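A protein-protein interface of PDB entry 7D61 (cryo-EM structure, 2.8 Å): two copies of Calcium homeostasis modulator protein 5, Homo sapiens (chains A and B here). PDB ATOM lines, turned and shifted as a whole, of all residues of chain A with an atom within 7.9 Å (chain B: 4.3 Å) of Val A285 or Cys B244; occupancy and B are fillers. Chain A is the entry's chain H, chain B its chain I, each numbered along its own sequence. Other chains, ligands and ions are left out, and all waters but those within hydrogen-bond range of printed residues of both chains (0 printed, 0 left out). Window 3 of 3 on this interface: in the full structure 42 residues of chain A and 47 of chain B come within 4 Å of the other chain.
Hydrophobic or aromatic side chains of chain B that line the printed part of chain A: Leu B242, Phe B245 and Pro B251. Of the 12 printed residues of chain A, 4 touch a printed residue of chain B. Among the printed residues, 8 pairs touch across the chains. Among the printed residues, Asp or Glu carboxylates within 4 Å of a Lys or Arg side-chain nitrogen of the other chain: Asp A286 with Arg B240.
The side-chain carboxylate (OD1) of Asp A286 is in salt-bridge range of the guanidinium group (NH2) of Arg B240, 2.4 Å away.
Cys B244 touches one residue of chain A. Of the printed residues of chain A, Leu B242 touches Leu A281. Printed residues of chain A within 4 Å of Phe B245: Leu A281 (3.9 Å). Printed residues of chain B within 4 Å of Leu A281: Leu B242 and Phe B245. Printed residues of chain A within 4 Å of Pro B251: Val A285. Of the printed residues of chain A, Asn B241 touches His A282 (3.4 Å) and Val A285 (3.7 Å). Val A284 touches none of the printed residues of chain B. Thr A280 touches none of the printed residues of chain B. The nearest printed residue of chain B that does not touch Leu A281 is Asn B241 (4.4 Å).
CD2 of Leu A281 touches CD2 of Leu B242, 3.8 Å away. Leu A281 touches Phe B245. His A282 touches Arg B240 (NE2 to NH2, 3.7 Å). His A282 touches Asn B241 (CD2 to ND2, 3.4 Å). CG2 of Val A285 touches O of Asn B241, 3.7 Å away. CB of Cys B244 touches CG1 of Val A285, 3.9 Å away. Val A285 touches Pro B251.
OG of Ser A279 is in hydrogen-bond range of N of His A282, at 3.0 Å. The guanidinium group (NH2) of Arg B240 is in hydrogen-bond range of the side-chain amide oxygen (OD1) of Asn B241 (3.5 Å). OG of Ser A279 lies close to N of Leu A281 (3.5 Å). The side-chain sulfur of Cys B244 lies within hydrogen-bond range of the backbone carbonyl oxygen of Arg B240, at 3.3 Å.
No position is printed for both chains.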
ATOM      1  N   ALA A 265       5.356 -16.031 -22.069  1.00  0.00           N
ATOM      2  CA  ALA A 265       6.413 -15.699 -23.011  1.00  0.00           C
ATOM      3  C   ALA A 265       7.782 -16.178 -22.554  1.00  0.00           C
ATOM      4  O   ALA A 265       8.770 -15.951 -23.259  1.00  0.00           O
ATOM      5  CB  ALA A 265       6.447 -14.189 -23.250  1.00  0.00           C
ATOM      6  N   HIS A 277       6.241 -21.613 -35.738  1.00  0.00           N
ATOM      7  CA  HIS A 277       6.568 -20.441 -34.942  1.00  0.00           C
ATOM      8  C   HIS A 277       8.048 -20.477 -34.597  1.00  0.00           C
ATOM      9  O   HIS A 277       8.583 -21.529 -34.235  1.00  0.00           O
ATOM     10  CB  HIS A 277       5.723 -20.390 -33.669  1.00  0.00           C
ATOM     11  CG  HIS A 277       4.249 -20.339 -33.924  1.00  0.00           C
ATOM     12  ND1 HIS A 277       3.367 -21.248 -33.381  1.00  0.00           N
ATOM     13  CD2 HIS A 277       3.503 -19.487 -34.665  1.00  0.00           C
ATOM     14  CE1 HIS A 277       2.141 -20.958 -33.776  1.00  0.00           C
ATOM     15  NE2 HIS A 277       2.195 -19.893 -34.556  1.00  0.00           N
ATOM     16  N   SER A 279       9.706 -18.514 -32.292  1.00  0.00           N
ATOM     17  CA  SER A 279      10.032 -18.256 -30.896  1.00  0.00           C
ATOM     18  C   SER A 279       8.791 -18.539 -30.062  1.00  0.00           C
ATOM     19  O   SER A 279       7.709 -18.799 -30.594  1.00  0.00           O
ATOM     20  CB  SER A 279      10.527 -16.822 -30.688  1.00  0.00           C
ATOM     21  OG  SER A 279       9.502 -15.883 -30.951  1.00  0.00           O
ATOM     22  N   THR A 280       8.949 -18.486 -28.743  1.00  0.00           N
ATOM     23  CA  THR A 280       7.810 -18.637 -27.851  1.00  0.00           C
ATOM     24  C   THR A 280       7.039 -17.339 -27.664  1.00  0.00           C
ATOM     25  O   THR A 280       5.896 -17.377 -27.202  1.00  0.00           O
ATOM     26  CB  THR A 280       8.261 -19.175 -26.488  1.00  0.00           C
ATOM     27  OG1 THR A 280       7.121 -19.349 -25.640  1.00  0.00           O
ATOM     28  CG2 THR A 280       9.240 -18.222 -25.826  1.00  0.00           C
ATOM     29  N   LEU A 281       7.634 -16.199 -28.016  1.00  0.00           N
ATOM     30  CA  LEU A 281       6.897 -14.946 -28.081  1.00  0.00           C
ATOM     31  C   LEU A 281       6.064 -14.859 -29.350  1.00  0.00           C
ATOM     32  O   LEU A 281       4.992 -14.244 -29.347  1.00  0.00           O
ATOM     33  CB  LEU A 281       7.867 -13.768 -28.002  1.00  0.00           C
ATOM     34  CG  LEU A 281       7.278 -12.370 -27.839  1.00  0.00           C
ATOM     35  CD1 LEU A 281       6.651 -12.227 -26.473  1.00  0.00           C
ATOM     36  CD2 LEU A 281       8.350 -11.324 -28.046  1.00  0.00           C
ATOM     37  N   HIS A 282       6.543 -15.469 -30.437  1.00  0.00           N
ATOM     38  CA  HIS A 282       5.774 -15.552 -31.672  1.00  0.00           C
ATOM     39  C   HIS A 282       4.553 -16.449 -31.508  1.00  0.00           C
ATOM     40  O   HIS A 282       3.536 -16.242 -32.175  1.00  0.00           O
ATOM     41  CB  HIS A 282       6.682 -16.061 -32.795  1.00  0.00           C
ATOM     42  CG  HIS A 282       6.060 -16.040 -34.157  1.00  0.00           C
ATOM     43  ND1 HIS A 282       6.489 -16.859 -35.178  1.00  0.00           N
ATOM     44  CD2 HIS A 282       5.064 -15.284 -34.677  1.00  0.00           C
ATOM     45  CE1 HIS A 282       5.774 -16.623 -36.262  1.00  0.00           C
ATOM     46  NE2 HIS A 282       4.901 -15.671 -35.985  1.00  0.00           N
ATOM     47  N   ARG A 283       4.624 -17.430 -30.608  1.00  0.00           N
ATOM     48  CA  ARG A 283       3.515 -18.359 -30.427  1.00  0.00           C
ATOM     49  C   ARG A 283       2.388 -17.752 -29.599  1.00  0.00           C
ATOM     50  O   ARG A 283       1.212 -18.005 -29.877  1.00  0.00           O
ATOM     51  CB  ARG A 283       4.016 -19.648 -29.780  1.00  0.00           C
ATOM     52  CG  ARG A 283       3.024 -20.791 -29.840  1.00  0.00           C
ATOM     53  CD  ARG A 283       3.487 -21.963 -29.000  1.00  0.00           C
ATOM     54  NE  ARG A 283       4.087 -21.522 -27.747  1.00  0.00           N
ATOM     55  CZ  ARG A 283       3.424 -21.402 -26.602  1.00  0.00           C
ATOM     56  NH1 ARG A 283       2.132 -21.689 -26.549  1.00  0.00           N
ATOM     57  NH2 ARG A 283       4.053 -20.994 -25.510  1.00  0.00           N
ATOM     58  N   VAL A 284       2.715 -16.949 -28.584  1.00  0.00           N
ATOM     59  CA  VAL A 284       1.666 -16.373 -27.746  1.00  0.00           C
ATOM     60  C   VAL A 284       1.007 -15.162 -28.395  1.00  0.00           C
ATOM     61  O   VAL A 284      -0.065 -14.738 -27.948  1.00  0.00           O
ATOM     62  CB  VAL A 284       2.199 -15.997 -26.352  1.00  0.00           C
ATOM     63  CG1 VAL A 284       2.918 -17.174 -25.726  1.00  0.00           C
ATOM     64  CG2 VAL A 284       3.116 -14.786 -26.421  1.00  0.00           C
ATOM     65  N   VAL A 285       1.613 -14.592 -29.435  1.00  0.00           N
ATOM     66  CA  VAL A 285       0.976 -13.503 -30.166  1.00  0.00           C
ATOM     67  C   VAL A 285       0.009 -14.057 -31.205  1.00  0.00           C
ATOM     68  O   VAL A 285      -1.121 -13.574 -31.342  1.00  0.00           O
ATOM     69  CB  VAL A 285       2.055 -12.597 -30.791  1.00  0.00           C
ATOM     70  CG1 VAL A 285       1.483 -11.706 -31.878  1.00  0.00           C
ATOM     71  CG2 VAL A 285       2.716 -11.755 -29.717  1.00  0.00           C
ATOM     72  N   ASP A 286       0.415 -15.113 -31.914  1.00  0.00           N
ATOM     73  CA  ASP A 286      -0.424 -15.699 -32.951  1.00  0.00           C
ATOM     74  C   ASP A 286      -1.574 -16.525 -32.389  1.00  0.00           C
ATOM     75  O   ASP A 286      -2.484 -16.883 -33.141  1.00  0.00           O
ATOM     76  CB  ASP A 286       0.424 -16.570 -33.878  1.00  0.00           C
ATOM     77  CG  ASP A 286       0.955 -15.807 -35.070  1.00  0.00           C
ATOM     78  OD1 ASP A 286       1.057 -14.566 -34.983  1.00  0.00           O
ATOM     79  OD2 ASP A 286       1.269 -16.446 -36.095  1.00  0.00           O
ATOM     80  N   ASN A 287      -1.554 -16.840 -31.095  1.00  0.00           N
ATOM     81  CA  ASN A 287      -2.600 -17.632 -30.463  1.00  0.00           C
ATOM     82  C   ASN A 287      -3.401 -16.832 -29.448  1.00  0.00           C
ATOM     83  O   ASN A 287      -4.633 -16.794 -29.522  1.00  0.00           O
ATOM     84  CB  ASN A 287      -1.980 -18.868 -29.790  1.00  0.00           C
ATOM     85  CG  ASN A 287      -3.008 -19.931 -29.438  1.00  0.00           C
ATOM     86  OD1 ASN A 287      -4.199 -19.784 -29.712  1.00  0.00           O
ATOM     87  ND2 ASN A 287      -2.543 -21.012 -28.823  1.00  0.00           N
ATOM     88  N   GLY A 288      -2.733 -16.188 -28.497  1.00  0.00           N
ATOM     89  CA  GLY A 288      -3.412 -15.397 -27.488  1.00  0.00           C
ATOM     90  C   GLY A 288      -3.728 -16.181 -26.231  1.00  0.00           C
ATOM     91  O   GLY A 288      -2.903 -16.957 -25.749  1.00  0.00           O
ATOM     92  N   ARG B 240       6.484  -6.741 -35.553  1.00  0.00           N
ATOM     93  CA  ARG B 240       5.080  -7.109 -35.432  1.00  0.00           C
ATOM     94  C   ARG B 240       4.806  -7.834 -34.121  1.00  0.00           C
ATOM     95  O   ARG B 240       3.738  -7.654 -33.526  1.00  0.00           O
ATOM     96  CB  ARG B 240       4.673  -7.979 -36.622  1.00  0.00           C
ATOM     97  CG  ARG B 240       3.195  -8.309 -36.699  1.00  0.00           C
ATOM     98  CD  ARG B 240       2.957  -9.557 -37.524  1.00  0.00           C
ATOM     99  NE  ARG B 240       3.090 -10.770 -36.724  1.00  0.00           N
ATOM    100  CZ  ARG B 240       2.269 -11.811 -36.804  1.00  0.00           C
ATOM    101  NH1 ARG B 240       1.254 -11.791 -37.654  1.00  0.00           N
ATOM    102  NH2 ARG B 240       2.465 -12.872 -36.038  1.00  0.00           N
ATOM    103  N   ASN B 241       5.759  -8.635 -33.646  1.00  0.00           N
ATOM    104  CA  ASN B 241       5.542  -9.445 -32.454  1.00  0.00           C
ATOM    105  C   ASN B 241       5.709  -8.648 -31.168  1.00  0.00           C
ATOM    106  O   ASN B 241       5.176  -9.046 -30.128  1.00  0.00           O
ATOM    107  CB  ASN B 241       6.500 -10.635 -32.449  1.00  0.00           C
ATOM    108  CG  ASN B 241       6.075 -11.729 -33.399  1.00  0.00           C
ATOM    109  OD1 ASN B 241       4.937 -11.759 -33.860  1.00  0.00           O
ATOM    110  ND2 ASN B 241       6.993 -12.637 -33.702  1.00  0.00           N
ATOM    111  N   LEU B 242       6.442  -7.538 -31.210  1.00  0.00           N
ATOM    112  CA  LEU B 242       6.692  -6.754 -30.007  1.00  0.00           C
ATOM    113  C   LEU B 242       5.692  -5.628 -29.803  1.00  0.00           C
ATOM    114  O   LEU B 242       5.579  -5.117 -28.685  1.00  0.00           O
ATOM    115  CB  LEU B 242       8.106  -6.173 -30.040  1.00  0.00           C
ATOM    116  CG  LEU B 242       9.207  -7.167 -29.683  1.00  0.00           C
ATOM    117  CD1 LEU B 242      10.562  -6.542 -29.883  1.00  0.00           C
ATOM    118  CD2 LEU B 242       9.041  -7.627 -28.251  1.00  0.00           C
ATOM    119  N   LYS B 243       4.970  -5.226 -30.847  1.00  0.00           N
ATOM    120  CA  LYS B 243       3.920  -4.230 -30.691  1.00  0.00           C
ATOM    121  C   LYS B 243       2.593  -4.850 -30.290  1.00  0.00           C
ATOM    122  O   LYS B 243       1.749  -4.163 -29.706  1.00  0.00           O
ATOM    123  CB  LYS B 243       3.746  -3.435 -31.986  1.00  0.00           C
ATOM    124  CG  LYS B 243       4.929  -2.548 -32.326  1.00  0.00           C
ATOM    125  CD  LYS B 243       4.498  -1.319 -33.108  1.00  0.00           C
ATOM    126  CE  LYS B 243       3.753  -1.695 -34.378  1.00  0.00           C
ATOM    127  NZ  LYS B 243       3.171  -0.502 -35.051  1.00  0.00           N
ATOM    128  N   CYS B 244       2.391  -6.128 -30.588  1.00  0.00           N
ATOM    129  CA  CYS B 244       1.186  -6.841 -30.192  1.00  0.00           C
ATOM    130  C   CYS B 244       1.311  -7.498 -28.826  1.00  0.00           C
ATOM    131  O   CYS B 244       0.358  -8.135 -28.371  1.00  0.00           O
ATOM    132  CB  CYS B 244       0.834  -7.897 -31.241  1.00  0.00           C
ATOM    133  SG  CYS B 244       0.522  -7.221 -32.885  1.00  0.00           S
ATOM    134  N   PHE B 245       2.458  -7.360 -28.165  1.00  0.00           N
ATOM    135  CA  PHE B 245       2.665  -7.900 -26.828  1.00  0.00           C
ATOM    136  C   PHE B 245       2.553  -6.827 -25.753  1.00  0.00           C
ATOM    137  O   PHE B 245       1.916  -7.048 -24.720  1.00  0.00           O
ATOM    138  CB  PHE B 245       4.034  -8.586 -26.742  1.00  0.00           C
ATOM    139  CG  PHE B 245       4.280  -9.284 -25.436  1.00  0.00           C
ATOM    140  CD1 PHE B 245       3.493 -10.356 -25.050  1.00  0.00           C
ATOM    141  CD2 PHE B 245       5.297  -8.866 -24.592  1.00  0.00           C
ATOM    142  CE1 PHE B 245       3.715 -10.999 -23.847  1.00  0.00           C
ATOM    143  CE2 PHE B 245       5.524  -9.505 -23.388  1.00  0.00           C
ATOM    144  CZ  PHE B 245       4.732 -10.572 -23.016  1.00  0.00           C
ATOM    145  N   PHE B 246       3.154  -5.661 -25.983  1.00  0.00           N
ATOM    146  CA  PHE B 246       3.107  -4.581 -25.009  1.00  0.00           C
ATOM    147  C   PHE B 246       1.814  -3.787 -25.072  1.00  0.00           C
ATOM    148  O   PHE B 246       1.478  -3.099 -24.102  1.00  0.00           O
ATOM    149  CB  PHE B 246       4.293  -3.643 -25.213  1.00  0.00           C
ATOM    150  CG  PHE B 246       5.574  -4.170 -24.652  1.00  0.00           C
ATOM    151  CD1 PHE B 246       5.914  -3.935 -23.331  1.00  0.00           C
ATOM    152  CD2 PHE B 246       6.435  -4.912 -25.445  1.00  0.00           C
ATOM    153  CE1 PHE B 246       7.094  -4.422 -22.811  1.00  0.00           C
ATOM    154  CE2 PHE B 246       7.614  -5.405 -24.932  1.00  0.00           C
ATOM    155  CZ  PHE B 246       7.942  -5.159 -23.613  1.00  0.00           C
ATOM    156  N   ASN B 248      -1.189  -5.372 -26.232  1.00  0.00           N
ATOM    157  CA  ASN B 248      -2.248  -6.389 -26.147  1.00  0.00           C
ATOM    158  C   ASN B 248      -3.213  -6.307 -27.330  1.00  0.00           C
ATOM    159  O   ASN B 248      -4.435  -6.308 -27.172  1.00  0.00           O
ATOM    160  CB  ASN B 248      -2.996  -6.304 -24.812  1.00  0.00           C
ATOM    161  CG  ASN B 248      -3.647  -7.615 -24.425  1.00  0.00           C
ATOM    162  OD1 ASN B 248      -3.551  -8.606 -25.146  1.00  0.00           O
ATOM    163  ND2 ASN B 248      -4.314  -7.627 -23.278  1.00  0.00           N
ATOM    164  N   LYS B 249      -2.648  -6.234 -28.529  1.00  0.00           N
ATOM    165  CA  LYS B 249      -3.424  -6.131 -29.752  1.00  0.00           C
ATOM    166  C   LYS B 249      -3.566  -7.502 -30.404  1.00  0.00           C
ATOM    167  O   LYS B 249      -3.039  -8.510 -29.928  1.00  0.00           O
ATOM    168  CB  LYS B 249      -2.771  -5.142 -30.718  1.00  0.00           C
ATOM    169  CG  LYS B 249      -2.998  -3.684 -30.378  1.00  0.00           C
ATOM    170  CD  LYS B 249      -2.081  -2.793 -31.199  1.00  0.00           C
ATOM    171  CE  LYS B 249      -2.697  -1.423 -31.428  1.00  0.00           C
ATOM    172  NZ  LYS B 249      -1.664  -0.396 -31.740  1.00  0.00           N
ATOM    173  N   PRO B 251      -2.778  -9.308 -34.160  1.00  0.00           N
ATOM    174  CA  PRO B 251      -1.875  -8.977 -35.263  1.00  0.00           C
ATOM    175  C   PRO B 251      -2.493  -9.202 -36.637  1.00  0.00           C
ATOM    176  O   PRO B 251      -3.423  -9.990 -36.821  1.00  0.00           O
ATOM    177  CB  PRO B 251      -0.701  -9.939 -35.037  1.00  0.00           C
ATOM    178  CG  PRO B 251      -1.317 -11.131 -34.379  1.00  0.00           C
ATOM    179  CD  PRO B 251      -2.583 -10.688 -33.682  1.00  0.00           C
